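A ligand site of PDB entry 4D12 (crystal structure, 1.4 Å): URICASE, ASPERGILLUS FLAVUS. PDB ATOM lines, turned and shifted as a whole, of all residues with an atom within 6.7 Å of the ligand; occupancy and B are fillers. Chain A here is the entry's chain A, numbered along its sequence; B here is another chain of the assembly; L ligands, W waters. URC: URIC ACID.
Water W3 bridges N9 of the ligand (2.9 Å) and NH1 of Arg 177 (3.3 Å). Water W1 lies within hydrogen-bond range of the side-chain hydroxyl (OG1) of Thr 58 of chain B, the side-chain amide nitrogen (ND2) of Asn 255 and a nitrogen (N9) of the ligand.
N of Thr 58 of chain B is in hydrogen-bond range of O24 of the ligand, at 3.3 Å. OG1 of Thr 58 of chain B sits at hydrogen-bond distance from O24 of the ligand. An oxygen (O11) of the ligand sits at hydrogen-bond distance from the backbone NH of Val 228, at 2.8 Å. The guanidinium group (NH2) of Arg 177 is in hydrogen-bond range of an oxygen (O11) of the ligand (2.8 Å). NE2 of Gln 229 sits at hydrogen-bond distance from O13 of the ligand, 2.9 Å away. The backbone NH (N) of Asp 59 of chain B sits at hydrogen-bond distance from an oxygen (O24) of the ligand (2.9 Å). A nitrogen (N3) of the ligand lies close to the side-chain amide nitrogen (ND2) of Asn 255 (3.3 Å).
CZ of Phe 160 touches C5 of the ligand, at 3.3 Å. Leu 171 touches the ligand. CA of Ser 227 touches O11 of the ligand, at 3.4 Å. CD1 of Ile 289 touches O13 of the ligand, at 3.9 Å. Tyr 9 of chain B touches the ligand (CD2 to O13, 3.7 Å). Ile 55 of chain B touches the ligand. Ala 57 of chain B touches the ligand. Hydrophobic or aromatic side chains within 4 Å of the ligand: Phe 160, Leu 171, Val 228, Ile 289, Tyr 9 of chain B, Ile 55 of chain B and Ala 57 of chain B. Of the 26 residues printed, 13 come within 4 Å of the ligand. Along chain A the residues within 4 Å of the ligand span positions 160 to 289. The nearest printed residue that does not touch the ligand is Lys 11 of chain B (4.2 Å).
The side-chain amino group (NZ) of Lys 11 of chain B is in hydrogen-bond range of the side-chain hydroxyl (OG1) of Thr 58 of chain B, at 2.8 Å. The backbone NH (N) of Arg 177 lies within hydrogen-bond range of the backbone carbonyl oxygen (O) of Ser 158, at 2.9 Å. N of Gln 229 sits close to OG of Ser 227, at 3.3 Å. O of Asn 255 is in hydrogen-bond range of NE2 of His 257. The backbone NH (N) of Asn 255 sits at hydrogen-bond distance from the backbone carbonyl oxygen (O) of Gly 287, at 2.8 Å. O of Ser 227 is in hydrogen-bond range of OG of Ser 225 (2.9 Å). OH of Tyr 9 of chain B lies within hydrogen-bond range of O of Val 56 of chain B (2.6 Å).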
ATOM      1  N   SER A 158      28.993 -17.515   6.363  1.00  0.00           N
ATOM      2  CA  SER A 158      28.084 -16.989   5.384  1.00  0.00           C
ATOM      3  C   SER A 158      26.691 -17.445   5.779  1.00  0.00           C
ATOM      4  O   SER A 158      26.507 -18.585   6.211  1.00  0.00           O
ATOM      5  CB  SER A 158      28.465 -17.518   4.001  1.00  0.00           C
ATOM      6  OG  SER A 158      27.501 -17.157   3.036  1.00  0.00           O
ATOM      7  N   GLN A 159      25.731 -16.534   5.627  1.00  0.00           N
ATOM      8  CA  GLN A 159      24.349 -16.778   6.014  1.00  0.00           C
ATOM      9  C   GLN A 159      23.433 -16.276   4.919  1.00  0.00           C
ATOM     10  O   GLN A 159      23.818 -15.424   4.111  1.00  0.00           O
ATOM     11  CB  GLN A 159      24.028 -16.039   7.314  1.00  0.00           C
ATOM     12  CG  GLN A 159      25.042 -16.316   8.409  1.00  0.00           C
ATOM     13  CD  GLN A 159      24.659 -15.711   9.732  1.00  0.00           C
ATOM     14  OE1 GLN A 159      23.484 -15.650  10.090  1.00  0.00           O
ATOM     15  NE2 GLN A 159      25.656 -15.250  10.476  1.00  0.00           N
ATOM     16  N   PHE A 160      22.203 -16.773   4.893  1.00  0.00           N
ATOM     17  CA  PHE A 160      21.207 -16.178   4.023  1.00  0.00           C
ATOM     18  C   PHE A 160      19.818 -16.493   4.541  1.00  0.00           C
ATOM     19  O   PHE A 160      19.284 -17.596   4.362  1.00  0.00           O
ATOM     20  CB  PHE A 160      21.379 -16.608   2.550  1.00  0.00           C
ATOM     21  CG  PHE A 160      20.566 -15.782   1.588  1.00  0.00           C
ATOM     22  CD1 PHE A 160      20.761 -14.406   1.490  1.00  0.00           C
ATOM     23  CD2 PHE A 160      19.586 -16.366   0.803  1.00  0.00           C
ATOM     24  CE1 PHE A 160      19.996 -13.648   0.628  1.00  0.00           C
ATOM     25  CE2 PHE A 160      18.820 -15.619  -0.066  1.00  0.00           C
ATOM     26  CZ  PHE A 160      19.017 -14.253  -0.151  1.00  0.00           C
ATOM     27  N   PHE A 163      14.947 -13.397   3.537  1.00  0.00           N
ATOM     28  CA  PHE A 163      14.558 -13.035   2.173  1.00  0.00           C
ATOM     29  C   PHE A 163      13.059 -13.231   1.977  1.00  0.00           C
ATOM     30  O   PHE A 163      12.381 -13.881   2.778  1.00  0.00           O
ATOM     31  CB  PHE A 163      15.382 -13.806   1.134  1.00  0.00           C
ATOM     32  CG  PHE A 163      15.384 -15.297   1.350  1.00  0.00           C
ATOM     33  CD1 PHE A 163      14.384 -16.101   0.828  1.00  0.00           C
ATOM     34  CD2 PHE A 163      16.395 -15.895   2.092  1.00  0.00           C
ATOM     35  CE1 PHE A 163      14.408 -17.473   1.016  1.00  0.00           C
ATOM     36  CE2 PHE A 163      16.399 -17.265   2.321  1.00  0.00           C
ATOM     37  CZ  PHE A 163      15.398 -18.048   1.794  1.00  0.00           C
ATOM     38  N   LEU A 171      13.427 -22.169  -1.072  1.00  0.00           N
ATOM     39  CA  LEU A 171      14.734 -22.139  -0.446  1.00  0.00           C
ATOM     40  C   LEU A 171      14.596 -22.021   1.070  1.00  0.00           C
ATOM     41  O   LEU A 171      13.914 -21.136   1.580  1.00  0.00           O
ATOM     42  CB  LEU A 171      15.533 -20.955  -0.959  1.00  0.00           C
ATOM     43  CG  LEU A 171      16.965 -20.794  -0.429  1.00  0.00           C
ATOM     44  CD1 LEU A 171      17.851 -21.942  -0.872  1.00  0.00           C
ATOM     45  CD2 LEU A 171      17.538 -19.467  -0.903  1.00  0.00           C
ATOM     46  N   ARG A 177      26.361 -21.451   5.804  1.00  0.00           N
ATOM     47  CA  ARG A 177      26.542 -22.054   4.492  1.00  0.00           C
ATOM     48  C   ARG A 177      27.933 -21.760   3.966  1.00  0.00           C
ATOM     49  O   ARG A 177      28.655 -20.922   4.509  1.00  0.00           O
ATOM     50  CB  ARG A 177      25.488 -21.525   3.493  1.00  0.00           C
ATOM     51  CG  ARG A 177      25.632 -20.046   3.183  1.00  0.00           C
ATOM     52  CD  ARG A 177      24.649 -19.529   2.147  1.00  0.00           C
ATOM     53  NE  ARG A 177      25.014 -18.162   1.793  1.00  0.00           N
ATOM     54  CZ  ARG A 177      24.416 -17.430   0.851  1.00  0.00           C
ATOM     55  NH1 ARG A 177      23.380 -17.887   0.162  1.00  0.00           N
ATOM     56  NH2 ARG A 177      24.876 -16.220   0.589  1.00  0.00           N
ATOM     57  N   LEU A 179      30.190 -20.128   1.010  1.00  0.00           N
ATOM     58  CA  LEU A 179      30.145 -19.095  -0.017  1.00  0.00           C
ATOM     59  C   LEU A 179      31.387 -19.183  -0.882  1.00  0.00           C
ATOM     60  O   LEU A 179      32.515 -19.118  -0.377  1.00  0.00           O
ATOM     61  CB  LEU A 179      30.032 -17.700   0.592  1.00  0.00           C
ATOM     62  CG  LEU A 179      30.004 -16.519  -0.389  1.00  0.00           C
ATOM     63  CD1 LEU A 179      28.817 -16.623  -1.328  1.00  0.00           C
ATOM     64  CD2 LEU A 179      29.974 -15.201   0.385  1.00  0.00           C
ATOM     65  N   SER A 225      28.889 -13.012   6.556  1.00  0.00           N
ATOM     66  CA  SER A 225      28.142 -12.417   5.459  1.00  0.00           C
ATOM     67  C   SER A 225      26.643 -12.640   5.568  1.00  0.00           C
ATOM     68  O   SER A 225      26.199 -13.764   5.701  1.00  0.00           O
ATOM     69  CB  SER A 225      28.618 -13.025   4.144  1.00  0.00           C
ATOM     70  OG  SER A 225      27.857 -12.598   3.044  1.00  0.00           O
ATOM     71  N   ALA A 226      25.896 -11.553   5.472  1.00  0.00           N
ATOM     72  CA  ALA A 226      24.440 -11.593   5.466  1.00  0.00           C
ATOM     73  C   ALA A 226      23.869 -11.970   4.102  1.00  0.00           C
ATOM     74  O   ALA A 226      22.721 -12.421   4.000  1.00  0.00           O
ATOM     75  CB  ALA A 226      23.877 -10.254   5.891  1.00  0.00           C
ATOM     76  N   SER A 227      24.673 -11.762   3.067  1.00  0.00           N
ATOM     77  CA  SER A 227      24.304 -12.010   1.678  1.00  0.00           C
ATOM     78  C   SER A 227      25.515 -11.612   0.844  1.00  0.00           C
ATOM     79  O   SER A 227      26.371 -10.868   1.300  1.00  0.00           O
ATOM     80  CB  SER A 227      23.110 -11.159   1.218  1.00  0.00           C
ATOM     81  OG  SER A 227      23.457  -9.786   1.225  1.00  0.00           O
ATOM     82  N   VAL A 228      25.548 -12.062  -0.401  1.00  0.00           N
ATOM     83  CA  VAL A 228      26.559 -11.583  -1.339  1.00  0.00           C
ATOM     84  C   VAL A 228      26.456 -10.049  -1.504  1.00  0.00           C
ATOM     85  O   VAL A 228      27.474  -9.336  -1.498  1.00  0.00           O
ATOM     86  CB  VAL A 228      26.469 -12.300  -2.695  1.00  0.00           C
ATOM     87  CG1 VAL A 228      27.485 -11.732  -3.678  1.00  0.00           C
ATOM     88  CG2 VAL A 228      26.709 -13.798  -2.516  1.00  0.00           C
ATOM     89  N   GLN A 229      25.222  -9.580  -1.612  1.00  0.00           N
ATOM     90  CA  GLN A 229      24.926  -8.151  -1.728  1.00  0.00           C
ATOM     91  C   GLN A 229      25.610  -7.329  -0.635  1.00  0.00           C
ATOM     92  O   GLN A 229      26.280  -6.324  -0.905  1.00  0.00           O
ATOM     93  CB  GLN A 229      23.392  -7.931  -1.662  1.00  0.00           C
ATOM     94  CG  GLN A 229      22.604  -8.360  -2.883  1.00  0.00           C
ATOM     95  CD  GLN A 229      22.175  -9.834  -2.889  1.00  0.00           C
ATOM     96  OE1 GLN A 229      22.785 -10.696  -2.252  1.00  0.00           O
ATOM     97  NE2 GLN A 229      21.128 -10.120  -3.634  1.00  0.00           N
ATOM     98  N   ASN A 255      27.192 -16.574  -7.265  1.00  0.00           N
ATOM     99  CA  ASN A 255      27.082 -17.393  -6.069  1.00  0.00           C
ATOM    100  C   ASN A 255      27.171 -18.834  -6.554  1.00  0.00           C
ATOM    101  O   ASN A 255      26.222 -19.343  -7.126  1.00  0.00           O
ATOM    102  CB  ASN A 255      25.778 -17.101  -5.347  1.00  0.00           C
ATOM    103  CG  ASN A 255      25.738 -17.677  -3.954  1.00  0.00           C
ATOM    104  OD1 ASN A 255      26.671 -18.323  -3.512  1.00  0.00           O
ATOM    105  ND2 ASN A 255      24.642 -17.438  -3.245  1.00  0.00           N
ATOM    106  N   HIS A 257      27.046 -22.339  -6.022  1.00  0.00           N
ATOM    107  CA  HIS A 257      26.367 -23.028  -4.924  1.00  0.00           C
ATOM    108  C   HIS A 257      27.037 -24.369  -4.615  1.00  0.00           C
ATOM    109  O   HIS A 257      27.434 -25.117  -5.518  1.00  0.00           O
ATOM    110  CB  HIS A 257      24.900 -23.251  -5.240  1.00  0.00           C
ATOM    111  CG  HIS A 257      24.165 -22.013  -5.610  1.00  0.00           C
ATOM    112  ND1 HIS A 257      23.966 -20.963  -4.730  1.00  0.00           N
ATOM    113  CD2 HIS A 257      23.593 -21.634  -6.775  1.00  0.00           C
ATOM    114  CE1 HIS A 257      23.280 -20.014  -5.347  1.00  0.00           C
ATOM    115  NE2 HIS A 257      23.049 -20.391  -6.582  1.00  0.00           N
ATOM    116  N   GLY A 287      23.593 -18.077  -8.765  1.00  0.00           N
ATOM    117  CA  GLY A 287      23.245 -16.709  -8.513  1.00  0.00           C
ATOM    118  C   GLY A 287      24.239 -15.797  -9.194  1.00  0.00           C
ATOM    119  O   GLY A 287      25.408 -16.146  -9.384  1.00  0.00           O
ATOM    120  N   ILE A 289      25.159 -11.625  -8.839  1.00  0.00           N
ATOM    121  CA  ILE A 289      24.861 -10.454  -8.010  1.00  0.00           C
ATOM    122  C   ILE A 289      25.780  -9.328  -8.480  1.00  0.00           C
ATOM    123  O   ILE A 289      26.990  -9.521  -8.579  1.00  0.00           O
ATOM    124  CB  ILE A 289      25.100 -10.751  -6.514  1.00  0.00           C
ATOM    125  CG1 ILE A 289      24.616 -12.158  -6.122  1.00  0.00           C
ATOM    126  CG2 ILE A 289      24.443  -9.667  -5.657  1.00  0.00           C
ATOM    127  CD1 ILE A 289      23.125 -12.396  -6.235  1.00  0.00           C
ATOM    128  N   TYR B   9      20.435  -8.283  -9.810  1.00  0.00           N
ATOM    129  CA  TYR B   9      20.833  -9.569  -9.272  1.00  0.00           C
ATOM    130  C   TYR B   9      19.799 -10.605  -9.724  1.00  0.00           C
ATOM    131  O   TYR B   9      18.642 -10.285 -10.040  1.00  0.00           O
ATOM    132  CB  TYR B   9      20.927  -9.517  -7.719  1.00  0.00           C
ATOM    133  CG  TYR B   9      19.569  -9.723  -7.128  1.00  0.00           C
ATOM    134  CD1 TYR B   9      18.599  -8.719  -7.198  1.00  0.00           C
ATOM    135  CD2 TYR B   9      19.191 -10.977  -6.669  1.00  0.00           C
ATOM    136  CE1 TYR B   9      17.305  -8.960  -6.775  1.00  0.00           C
ATOM    137  CE2 TYR B   9      17.905 -11.204  -6.231  1.00  0.00           C
ATOM    138  CZ  TYR B   9      16.966 -10.199  -6.312  1.00  0.00           C
ATOM    139  OH  TYR B   9      15.675 -10.437  -5.931  1.00  0.00           O
ATOM    140  N   GLY B  10      20.206 -11.855  -9.759  1.00  0.00           N
ATOM    141  CA  GLY B  10      19.279 -12.913 -10.118  1.00  0.00           C
ATOM    142  C   GLY B  10      19.972 -14.222 -10.367  1.00  0.00           C
ATOM    143  O   GLY B  10      20.954 -14.526  -9.717  1.00  0.00           O
ATOM    144  N   LYS B  11      19.429 -15.020 -11.289  1.00  0.00           N
ATOM    145  CA  LYS B  11      19.963 -16.353 -11.538  1.00  0.00           C
ATOM    146  C   LYS B  11      20.430 -16.432 -12.967  1.00  0.00           C
ATOM    147  O   LYS B  11      19.707 -16.067 -13.897  1.00  0.00           O
ATOM    148  CB  LYS B  11      18.916 -17.453 -11.263  1.00  0.00           C
ATOM    149  CG  LYS B  11      19.532 -18.836 -11.082  1.00  0.00           C
ATOM    150  CD  LYS B  11      20.284 -18.967  -9.767  1.00  0.00           C
ATOM    151  CE  LYS B  11      19.653 -19.873  -8.755  1.00  0.00           C
ATOM    152  NZ  LYS B  11      20.261 -19.708  -7.407  1.00  0.00           N
ATOM    153  N   ASN B  52      17.448  -8.294   3.766  1.00  0.00           N
ATOM    154  CA  ASN B  52      17.097  -9.291   2.770  1.00  0.00           C
ATOM    155  C   ASN B  52      15.614  -9.325   2.435  1.00  0.00           C
ATOM    156  O   ASN B  52      15.233 -10.011   1.497  1.00  0.00           O
ATOM    157  CB  ASN B  52      17.608 -10.669   3.185  1.00  0.00           C
ATOM    158  CG  ASN B  52      19.122 -10.775   3.074  1.00  0.00           C
ATOM    159  OD1 ASN B  52      19.746 -10.083   2.249  1.00  0.00           O
ATOM    160  ND2 ASN B  52      19.721 -11.667   3.857  1.00  0.00           N
ATOM    161  N   ILE B  55      14.791  -8.951  -1.147  1.00  0.00           N
ATOM    162  CA  ILE B  55      15.337  -9.906  -2.113  1.00  0.00           C
ATOM    163  C   ILE B  55      14.342 -11.027  -2.389  1.00  0.00           C
ATOM    164  O   ILE B  55      13.980 -11.806  -1.504  1.00  0.00           O
ATOM    165  CB  ILE B  55      16.689 -10.473  -1.652  1.00  0.00           C
ATOM    166  CG1 ILE B  55      17.736  -9.347  -1.599  1.00  0.00           C
ATOM    167  CG2 ILE B  55      17.150 -11.584  -2.585  1.00  0.00           C
ATOM    168  CD1 ILE B  55      17.913  -8.574  -2.884  1.00  0.00           C
ATOM    169  N   VAL B  56      13.932 -11.100  -3.643  1.00  0.00           N
ATOM    170  CA  VAL B  56      13.348 -12.313  -4.216  1.00  0.00           C
ATOM    171  C   VAL B  56      14.514 -13.259  -4.468  1.00  0.00           C
ATOM    172  O   VAL B  56      15.393 -12.958  -5.278  1.00  0.00           O
ATOM    173  CB  VAL B  56      12.608 -11.991  -5.534  1.00  0.00           C
ATOM    174  CG1 VAL B  56      12.036 -13.253  -6.165  1.00  0.00           C
ATOM    175  CG2 VAL B  56      11.491 -10.982  -5.260  1.00  0.00           C
ATOM    176  N   ALA B  57      14.584 -14.352  -3.727  1.00  0.00           N
ATOM    177  CA  ALA B  57      15.782 -15.191  -3.764  1.00  0.00           C
ATOM    178  C   ALA B  57      16.073 -15.626  -5.185  1.00  0.00           C
ATOM    179  O   ALA B  57      15.153 -15.913  -5.962  1.00  0.00           O
ATOM    180  CB  ALA B  57      15.622 -16.417  -2.872  1.00  0.00           C
ATOM    181  N   THR B  58      17.351 -15.698  -5.527  1.00  0.00           N
ATOM    182  CA  THR B  58      17.716 -16.202  -6.853  1.00  0.00           C
ATOM    183  C   THR B  58      17.164 -17.614  -7.093  1.00  0.00           C
ATOM    184  O   THR B  58      16.752 -17.962  -8.200  1.00  0.00           O
ATOM    185  CB  THR B  58      19.227 -16.111  -7.138  1.00  0.00           C
ATOM    186  OG1 THR B  58      19.957 -17.087  -6.391  1.00  0.00           O
ATOM    187  CG2 THR B  58      19.781 -14.699  -6.848  1.00  0.00           C
ATOM    188  N   ASP B  59      17.119 -18.425  -6.027  1.00  0.00           N
ATOM    189  CA  ASP B  59      16.503 -19.737  -6.131  1.00  0.00           C
ATOM    190  C   ASP B  59      15.035 -19.666  -6.523  1.00  0.00           C
ATOM    191  O   ASP B  59      14.537 -20.502  -7.288  1.00  0.00           O
ATOM    192  CB  ASP B  59      16.649 -20.483  -4.803  1.00  0.00           C
ATOM    193  CG  ASP B  59      16.211 -21.926  -4.914  1.00  0.00           C
ATOM    194  OD1 ASP B  59      16.996 -22.734  -5.461  1.00  0.00           O
ATOM    195  OD2 ASP B  59      15.082 -22.259  -4.510  1.00  0.00           O
ATOM    196  N   SER B  60      14.331 -18.681  -5.988  1.00  0.00           N
ATOM    197  CA  SER B  60      12.930 -18.441  -6.364  1.00  0.00           C
ATOM    198  C   SER B  60      12.779 -17.966  -7.801  1.00  0.00           C
ATOM    199  O   SER B  60      11.830 -18.322  -8.471  1.00  0.00           O
ATOM    200  CB  SER B  60      12.284 -17.430  -5.404  1.00  0.00           C
ATOM    201  OG  SER B  60      12.434 -17.861  -4.057  1.00  0.00           O
HETATM  202  N1  URC L   1      21.970 -13.548  -2.297  1.00  0.00           N
HETATM  203  C2  URC L   1      22.707 -14.510  -1.598  1.00  0.00           C
HETATM  204  C6  URC L   1      20.827 -13.778  -3.026  1.00  0.00           C
HETATM  205  N3  URC L   1      22.313 -15.805  -1.619  1.00  0.00           N
HETATM  206  O11 URC L   1      23.684 -14.142  -0.953  1.00  0.00           O
HETATM  207  C4  URC L   1      21.239 -16.094  -2.317  1.00  0.00           C
HETATM  208  C5  URC L   1      20.431 -15.162  -3.030  1.00  0.00           C
HETATM  209  N9  URC L   1      20.658 -17.312  -2.541  1.00  0.00           N
HETATM  210  O13 URC L   1      20.258 -12.845  -3.598  1.00  0.00           O
HETATM  211  N7  URC L   1      19.389 -15.775  -3.630  1.00  0.00           N
HETATM  212  C8  URC L   1      19.537 -17.097  -3.343  1.00  0.00           C
HETATM  213  O24 URC L   1      18.854 -18.040  -3.767  1.00  0.00           O
HETATM  214  O   HOH W   1      22.413 -16.354  -5.223  1.00  0.00           O
HETATM  215  O   HOH W   2      20.065 -20.339  -3.813  1.00  0.00           O
HETATM  216  O   HOH W   3      21.702 -19.893  -1.807  1.00  0.00           O
